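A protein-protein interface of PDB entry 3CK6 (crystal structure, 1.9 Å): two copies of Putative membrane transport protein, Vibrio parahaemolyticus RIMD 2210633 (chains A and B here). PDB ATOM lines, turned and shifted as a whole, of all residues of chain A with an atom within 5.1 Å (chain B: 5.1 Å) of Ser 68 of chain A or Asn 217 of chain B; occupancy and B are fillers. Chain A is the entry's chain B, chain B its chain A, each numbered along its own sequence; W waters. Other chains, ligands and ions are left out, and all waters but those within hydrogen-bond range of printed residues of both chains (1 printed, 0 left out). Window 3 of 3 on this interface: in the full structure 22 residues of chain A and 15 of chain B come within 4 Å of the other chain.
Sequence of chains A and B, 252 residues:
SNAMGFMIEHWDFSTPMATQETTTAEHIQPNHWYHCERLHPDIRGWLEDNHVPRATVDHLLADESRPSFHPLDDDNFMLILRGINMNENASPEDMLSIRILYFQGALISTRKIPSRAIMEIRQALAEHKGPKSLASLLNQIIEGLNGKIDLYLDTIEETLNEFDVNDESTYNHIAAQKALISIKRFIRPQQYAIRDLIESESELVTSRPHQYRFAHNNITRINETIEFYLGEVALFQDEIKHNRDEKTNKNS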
ATOM      1  N   HIS A  59      31.764   6.750  26.059  1.00  0.00           N
ATOM      2  CA  HIS A  59      30.531   7.024  25.307  1.00  0.00           C
ATOM      3  C   HIS A  59      30.475   6.168  24.036  1.00  0.00           C
ATOM      4  O   HIS A  59      29.414   5.644  23.663  1.00  0.00           O
ATOM      5  CB  HIS A  59      30.350   8.520  24.985  1.00  0.00           C
ATOM      6  CG  HIS A  59      28.917   8.935  24.790  1.00  0.00           C
ATOM      7  ND1 HIS A  59      28.430   9.392  23.583  1.00  0.00           N
ATOM      8  CD2 HIS A  59      27.863   8.945  25.642  1.00  0.00           C
ATOM      9  CE1 HIS A  59      27.142   9.672  23.701  1.00  0.00           C
ATOM     10  NE2 HIS A  59      26.777   9.424  24.944  1.00  0.00           N
ATOM     11  N   ARG A  66      21.916   6.690  21.188  1.00  0.00           N
ATOM     12  CA  ARG A  66      21.000   7.216  20.188  1.00  0.00           C
ATOM     13  C   ARG A  66      21.820   7.864  19.066  1.00  0.00           C
ATOM     14  O   ARG A  66      22.937   8.364  19.310  1.00  0.00           O
ATOM     15  CB  ARG A  66      20.054   8.242  20.831  1.00  0.00           C
ATOM     16  CG  ARG A  66      20.789   9.516  21.274  1.00  0.00           C
ATOM     17  CD  ARG A  66      19.850  10.519  21.911  1.00  0.00           C
ATOM     18  NE  ARG A  66      19.002  11.225  20.949  1.00  0.00           N
ATOM     19  CZ  ARG A  66      19.299  12.398  20.400  1.00  0.00           C
ATOM     20  NH1 ARG A  66      20.440  13.019  20.703  1.00  0.00           N
ATOM     21  NH2 ARG A  66      18.437  12.962  19.560  1.00  0.00           N
ATOM     22  N   PRO A  67      21.281   7.867  17.828  1.00  0.00           N
ATOM     23  CA  PRO A  67      21.965   8.628  16.788  1.00  0.00           C
ATOM     24  C   PRO A  67      22.170  10.064  17.242  1.00  0.00           C
ATOM     25  O   PRO A  67      21.279  10.667  17.842  1.00  0.00           O
ATOM     26  CB  PRO A  67      21.013   8.543  15.592  1.00  0.00           C
ATOM     27  CG  PRO A  67      20.285   7.241  15.844  1.00  0.00           C
ATOM     28  CD  PRO A  67      20.071   7.205  17.310  1.00  0.00           C
ATOM     29  N   SER A  68      23.369  10.574  16.994  1.00  0.00           N
ATOM     30  CA  SER A  68      23.785  11.885  17.502  1.00  0.00           C
ATOM     31  C   SER A  68      25.134  12.276  16.933  1.00  0.00           C
ATOM     32  O   SER A  68      25.893  11.414  16.477  1.00  0.00           O
ATOM     33  CB  SER A  68      23.846  11.882  19.034  1.00  0.00           C
ATOM     34  OG  SER A  68      24.512  10.724  19.502  1.00  0.00           O
ATOM     35  N   PHE A  69      25.419  13.579  16.984  1.00  0.00           N
ATOM     36  CA  PHE A  69      26.698  14.145  16.567  1.00  0.00           C
ATOM     37  C   PHE A  69      27.328  14.863  17.748  1.00  0.00           C
ATOM     38  O   PHE A  69      26.685  15.658  18.420  1.00  0.00           O
ATOM     39  CB  PHE A  69      26.537  15.106  15.375  1.00  0.00           C
ATOM     40  CG  PHE A  69      27.790  15.900  15.065  1.00  0.00           C
ATOM     41  CD1 PHE A  69      28.838  15.312  14.345  1.00  0.00           C
ATOM     42  CD2 PHE A  69      27.931  17.206  15.502  1.00  0.00           C
ATOM     43  CE1 PHE A  69      30.000  16.018  14.051  1.00  0.00           C
ATOM     44  CE2 PHE A  69      29.124  17.922  15.233  1.00  0.00           C
ATOM     45  CZ  PHE A  69      30.148  17.312  14.514  1.00  0.00           C
ATOM     46  N   HIS A  70      28.598  14.576  17.994  1.00  0.00           N
ATOM     47  CA  HIS A  70      29.333  15.186  19.113  1.00  0.00           C
ATOM     48  C   HIS A  70      30.625  15.833  18.621  1.00  0.00           C
ATOM     49  O   HIS A  70      31.561  15.109  18.288  1.00  0.00           O
ATOM     50  CB  HIS A  70      29.663  14.109  20.170  1.00  0.00           C
ATOM     51  CG  HIS A  70      28.466  13.323  20.614  1.00  0.00           C
ATOM     52  ND1 HIS A  70      27.818  13.564  21.805  1.00  0.00           N
ATOM     53  CD2 HIS A  70      27.779  12.324  20.006  1.00  0.00           C
ATOM     54  CE1 HIS A  70      26.788  12.739  21.915  1.00  0.00           C
ATOM     55  NE2 HIS A  70      26.741  11.979  20.835  1.00  0.00           N
ATOM     56  N   MET A  78      32.463  12.632  17.151  1.00  0.00           N
ATOM     57  CA  MET A  78      31.851  11.314  17.176  1.00  0.00           C
ATOM     58  C   MET A  78      30.488  11.435  16.521  1.00  0.00           C
ATOM     59  O   MET A  78      29.754  12.405  16.758  1.00  0.00           O
ATOM     60  CB  MET A  78      31.697  10.801  18.615  1.00  0.00           C
ATOM     61  CG  MET A  78      31.070   9.405  18.726  1.00  0.00           C
ATOM     62  SD  MET A  78      30.755   8.869  20.575  1.00  0.00           S
ATOM     63  CE  MET A  78      32.491   9.394  21.314  1.00  0.00           C
ATOM     64  N   LEU A  79      30.181  10.467  15.665  1.00  0.00           N
ATOM     65  CA  LEU A  79      28.917  10.430  14.998  1.00  0.00           C
ATOM     66  C   LEU A  79      28.337   9.029  15.215  1.00  0.00           C
ATOM     67  O   LEU A  79      29.004   8.012  14.968  1.00  0.00           O
ATOM     68  CB  LEU A  79      29.055  10.768  13.502  1.00  0.00           C
ATOM     69  CG  LEU A  79      27.763  10.555  12.665  1.00  0.00           C
ATOM     70  CD1 LEU A  79      26.714  11.648  12.985  1.00  0.00           C
ATOM     71  CD2 LEU A  79      28.096  10.594  11.195  1.00  0.00           C
ATOM     72  N   ILE A  80      27.118   8.978  15.723  1.00  0.00           N
ATOM     73  CA  ILE A  80      26.433   7.702  15.957  1.00  0.00           C
ATOM     74  C   ILE A  80      25.181   7.592  15.055  1.00  0.00           C
ATOM     75  O   ILE A  80      24.418   8.544  14.949  1.00  0.00           O
ATOM     76  CB  ILE A  80      26.101   7.540  17.467  1.00  0.00           C
ATOM     77  CG1 ILE A  80      27.404   7.586  18.291  1.00  0.00           C
ATOM     78  CG2 ILE A  80      25.265   6.245  17.771  1.00  0.00           C
ATOM     79  CD1 ILE A  80      27.190   7.833  19.771  1.00  0.00           C
ATOM     80  N   PRO A 189      16.008  10.945  15.386  1.00  0.00           N
ATOM     81  CA  PRO A 189      17.334  11.475  15.772  1.00  0.00           C
ATOM     82  C   PRO A 189      18.423  11.370  14.679  1.00  0.00           C
ATOM     83  O   PRO A 189      19.317  12.205  14.645  1.00  0.00           O
ATOM     84  CB  PRO A 189      17.725  10.652  17.006  1.00  0.00           C
ATOM     85  CG  PRO A 189      16.718   9.606  17.175  1.00  0.00           C
ATOM     86  CD  PRO A 189      15.515   9.925  16.328  1.00  0.00           C
ATOM     87  N   ALA A 193      21.122  14.271  13.720  1.00  0.00           N
ATOM     88  CA  ALA A 193      22.568  13.977  13.776  1.00  0.00           C
ATOM     89  C   ALA A 193      23.240  14.461  12.497  1.00  0.00           C
ATOM     90  O   ALA A 193      24.285  15.133  12.544  1.00  0.00           O
ATOM     91  CB  ALA A 193      22.794  12.500  13.942  1.00  0.00           C
ATOM     92  N   TYR B 212      29.746  16.794  29.573  1.00  0.00           N
ATOM     93  CA  TYR B 212      28.395  17.287  29.784  1.00  0.00           C
ATOM     94  C   TYR B 212      27.517  17.111  28.542  1.00  0.00           C
ATOM     95  O   TYR B 212      26.379  16.826  28.657  1.00  0.00           O
ATOM     96  CB  TYR B 212      28.329  18.696  30.397  1.00  0.00           C
ATOM     97  CG  TYR B 212      28.501  18.780  31.894  1.00  0.00           C
ATOM     98  CD1 TYR B 212      29.728  18.930  32.421  1.00  0.00           C
ATOM     99  CD2 TYR B 212      27.435  18.699  32.786  1.00  0.00           C
ATOM    100  CE1 TYR B 212      29.942  19.008  33.726  1.00  0.00           C
ATOM    101  CE2 TYR B 212      27.657  18.796  34.166  1.00  0.00           C
ATOM    102  CZ  TYR B 212      28.937  18.952  34.627  1.00  0.00           C
ATOM    103  OH  TYR B 212      29.344  19.064  35.957  1.00  0.00           O
ATOM    104  N   ARG B 213      28.064  17.226  27.363  1.00  0.00           N
ATOM    105  CA  ARG B 213      27.251  16.947  26.166  1.00  0.00           C
ATOM    106  C   ARG B 213      26.852  15.466  26.075  1.00  0.00           C
ATOM    107  O   ARG B 213      25.743  15.158  25.628  1.00  0.00           O
ATOM    108  CB  ARG B 213      27.901  17.413  24.864  1.00  0.00           C
ATOM    109  CG  ARG B 213      28.543  18.810  24.894  1.00  0.00           C
ATOM    110  CD  ARG B 213      27.562  19.989  24.856  1.00  0.00           C
ATOM    111  NE  ARG B 213      28.295  21.253  24.711  1.00  0.00           N
ATOM    112  CZ  ARG B 213      29.079  21.790  25.648  1.00  0.00           C
ATOM    113  NH1 ARG B 213      29.699  22.944  25.414  1.00  0.00           N
ATOM    114  NH2 ARG B 213      29.242  21.180  26.823  1.00  0.00           N
ATOM    115  N   PHE B 214      27.741  14.555  26.490  1.00  0.00           N
ATOM    116  CA  PHE B 214      27.333  13.131  26.632  1.00  0.00           C
ATOM    117  C   PHE B 214      26.165  12.949  27.622  1.00  0.00           C
ATOM    118  O   PHE B 214      25.247  12.202  27.350  1.00  0.00           O
ATOM    119  CB  PHE B 214      28.489  12.206  27.064  1.00  0.00           C
ATOM    120  CG  PHE B 214      29.717  12.251  26.177  1.00  0.00           C
ATOM    121  CD1 PHE B 214      29.620  12.394  24.792  1.00  0.00           C
ATOM    122  CD2 PHE B 214      30.983  12.062  26.742  1.00  0.00           C
ATOM    123  CE1 PHE B 214      30.784  12.397  23.986  1.00  0.00           C
ATOM    124  CE2 PHE B 214      32.140  12.082  25.948  1.00  0.00           C
ATOM    125  CZ  PHE B 214      32.037  12.250  24.573  1.00  0.00           C
ATOM    126  N   ALA B 215      26.219  13.611  28.775  1.00  0.00           N
ATOM    127  CA  ALA B 215      25.154  13.502  29.784  1.00  0.00           C
ATOM    128  C   ALA B 215      23.841  14.024  29.218  1.00  0.00           C
ATOM    129  O   ALA B 215      22.790  13.423  29.432  1.00  0.00           O
ATOM    130  CB  ALA B 215      25.523  14.280  31.048  1.00  0.00           C
ATOM    131  N   HIS B 216      23.916  15.120  28.470  1.00  0.00           N
ATOM    132  CA  HIS B 216      22.747  15.691  27.812  1.00  0.00           C
ATOM    133  C   HIS B 216      22.186  14.735  26.743  1.00  0.00           C
ATOM    134  O   HIS B 216      20.962  14.601  26.584  1.00  0.00           O
ATOM    135  CB  HIS B 216      23.038  17.071  27.227  1.00  0.00           C
ATOM    136  CG  HIS B 216      21.820  17.748  26.671  1.00  0.00           C
ATOM    137  ND1 HIS B 216      21.769  18.259  25.394  1.00  0.00           N
ATOM    138  CD2 HIS B 216      20.595  17.960  27.209  1.00  0.00           C
ATOM    139  CE1 HIS B 216      20.569  18.767  25.173  1.00  0.00           C
ATOM    140  NE2 HIS B 216      19.837  18.595  26.258  1.00  0.00           N
ATOM    141  N   ASN B 217      23.085  14.054  26.040  1.00  0.00           N
ATOM    142  CA  ASN B 217      22.700  13.067  25.056  1.00  0.00           C
ATOM    143  C   ASN B 217      21.987  11.867  25.719  1.00  0.00           C
ATOM    144  O   ASN B 217      21.003  11.371  25.185  1.00  0.00           O
ATOM    145  CB  ASN B 217      23.913  12.620  24.236  1.00  0.00           C
ATOM    146  CG  ASN B 217      23.518  11.815  23.004  1.00  0.00           C
ATOM    147  OD1 ASN B 217      22.643  12.222  22.231  1.00  0.00           O
ATOM    148  ND2 ASN B 217      24.194  10.696  22.791  1.00  0.00           N
ATOM    149  N   ASN B 218      22.470  11.434  26.881  1.00  0.00           N
ATOM    150  CA  ASN B 218      21.830  10.324  27.619  1.00  0.00           C
ATOM    151  C   ASN B 218      20.431  10.669  28.108  1.00  0.00           C
ATOM    152  O   ASN B 218      19.530   9.837  28.029  1.00  0.00           O
ATOM    153  CB  ASN B 218      22.720   9.876  28.786  1.00  0.00           C
ATOM    154  CG  ASN B 218      23.895   9.049  28.322  1.00  0.00           C
ATOM    155  OD1 ASN B 218      23.764   8.235  27.417  1.00  0.00           O
ATOM    156  ND2 ASN B 218      25.062   9.239  28.959  1.00  0.00           N
ATOM    157  N   ILE B 219      20.245  11.891  28.610  1.00  0.00           N
ATOM    158  CA  ILE B 219      18.921  12.325  29.072  1.00  0.00           C
ATOM    159  C   ILE B 219      17.937  12.480  27.896  1.00  0.00           C
ATOM    160  O   ILE B 219      16.768  12.088  28.019  1.00  0.00           O
ATOM    161  CB  ILE B 219      18.933  13.552  30.031  1.00  0.00           C
ATOM    162  CG1 ILE B 219      17.537  13.753  30.675  1.00  0.00           C
ATOM    163  CG2 ILE B 219      19.332  14.844  29.315  1.00  0.00           C
ATOM    164  CD1 ILE B 219      17.102  12.571  31.595  1.00  0.00           C
ATOM    165  N   THR B 220      18.436  12.987  26.767  1.00  0.00           N
ATOM    166  CA  THR B 220      17.620  13.069  25.536  1.00  0.00           C
ATOM    167  C   THR B 220      17.184  11.646  25.125  1.00  0.00           C
ATOM    168  O   THR B 220      16.004  11.413  24.816  1.00  0.00           O
ATOM    169  CB  THR B 220      18.361  13.777  24.396  1.00  0.00           C
ATOM    170  OG1 THR B 220      18.779  15.097  24.828  1.00  0.00           O
ATOM    171  CG2 THR B 220      17.425  13.916  23.141  1.00  0.00           C
ATOM    172  N   ARG B 221      18.137  10.710  25.126  1.00  0.00           N
ATOM    173  CA  ARG B 221      17.841   9.300  24.810  1.00  0.00           C
ATOM    174  C   ARG B 221      16.749   8.727  25.700  1.00  0.00           C
ATOM    175  O   ARG B 221      15.821   8.091  25.214  1.00  0.00           O
ATOM    176  CB  ARG B 221      19.104   8.424  24.929  1.00  0.00           C
ATOM    177  CG  ARG B 221      18.832   6.936  24.672  1.00  0.00           C
ATOM    178  CD  ARG B 221      20.109   6.089  24.768  1.00  0.00           C
ATOM    179  NE  ARG B 221      20.892   6.417  25.968  1.00  0.00           N
ATOM    180  CZ  ARG B 221      20.545   6.080  27.209  1.00  0.00           C
ATOM    181  NH1 ARG B 221      21.327   6.438  28.220  1.00  0.00           N
ATOM    182  NH2 ARG B 221      19.436   5.369  27.446  1.00  0.00           N
HETATM  183  O   HOH W   1      24.648   7.762  22.295  1.00  0.00           O
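Of chain A, only His 59, Arg 66, Ser 68 and His 70 come within 4 Å of Asn 217 of chain B.
Of the printed residues of chain A, Phe 214 of chain B touches His 59 (3.4 Å) and His 70 (3.7 Å).
Of the printed residues of chain A, Thr 220 of chain B touches Arg 66 (3.7 Å).
Of the printed residues of chain B, Arg 66 of chain A touches Asn 217, Thr 220 and Arg 221.
Of the printed residues of chain A, Arg 221 of chain B touches Arg 66 (3.6 Å).
The nearest printed residue of chain B that does not touch Ser 68 of chain A is Phe 214 of chain B (7.5 Å).
No position is printed for both chains.
Water W1 lies within hydrogen-bond range of ND2 of Asn 217 of chain B and N of Arg 66 of chain A.
OD1 of Asn 217 of chain B sits at hydrogen-bond distance from NH1 of Arg 66 of chain A (2.8 Å).
The side-chain hydroxyl of Ser 68 of chain A lies within hydrogen-bond range of the side-chain amide nitrogen of Asn 217 of chain B (3.3 Å).
ND2 of Asn 217 of chain B sits close to NE2 of His 70 of chain A.
Among the printed residues, pairs that only touch across the chains: His 59 of chain A with Phe 214 of chain B (3.4 Å), His 59 of chain A with Asn 217 of chain B (3.3 Å), Arg 66 of chain A with Thr 220 of chain B (3.7 Å), Arg 66 of chain A with Arg 221 of chain B (3.6 Å) and His 70 of chain A with Phe 214 of chain B (3.7 Å).
The backbone carbonyl oxygen (O) of His 216 of chain B is in hydrogen-bond range of the side-chain hydroxyl (OG1) of Thr 220 of chain B, at 2.8 Å.
OD1 of Asn 218 of chain B is in hydrogen-bond range of NH1 of Arg 221 of chain B (3.1 Å).
The backbone carbonyl oxygen (O) of Arg 66 of chain A sits at hydrogen-bond distance from the side-chain hydroxyl (OG) of Ser 68 of chain A.
OG of Ser 68 of chain A sits at hydrogen-bond distance from NE2 of His 70 of chain A, at 2.9 Å.
O of Ser 68 of chain A lies within hydrogen-bond range of N of Ile 80 of chain A (2.8 Å).
The backbone NH of His 70 of chain A lies within hydrogen-bond range of the backbone carbonyl oxygen of Met 78 of chain A (2.8 Å).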
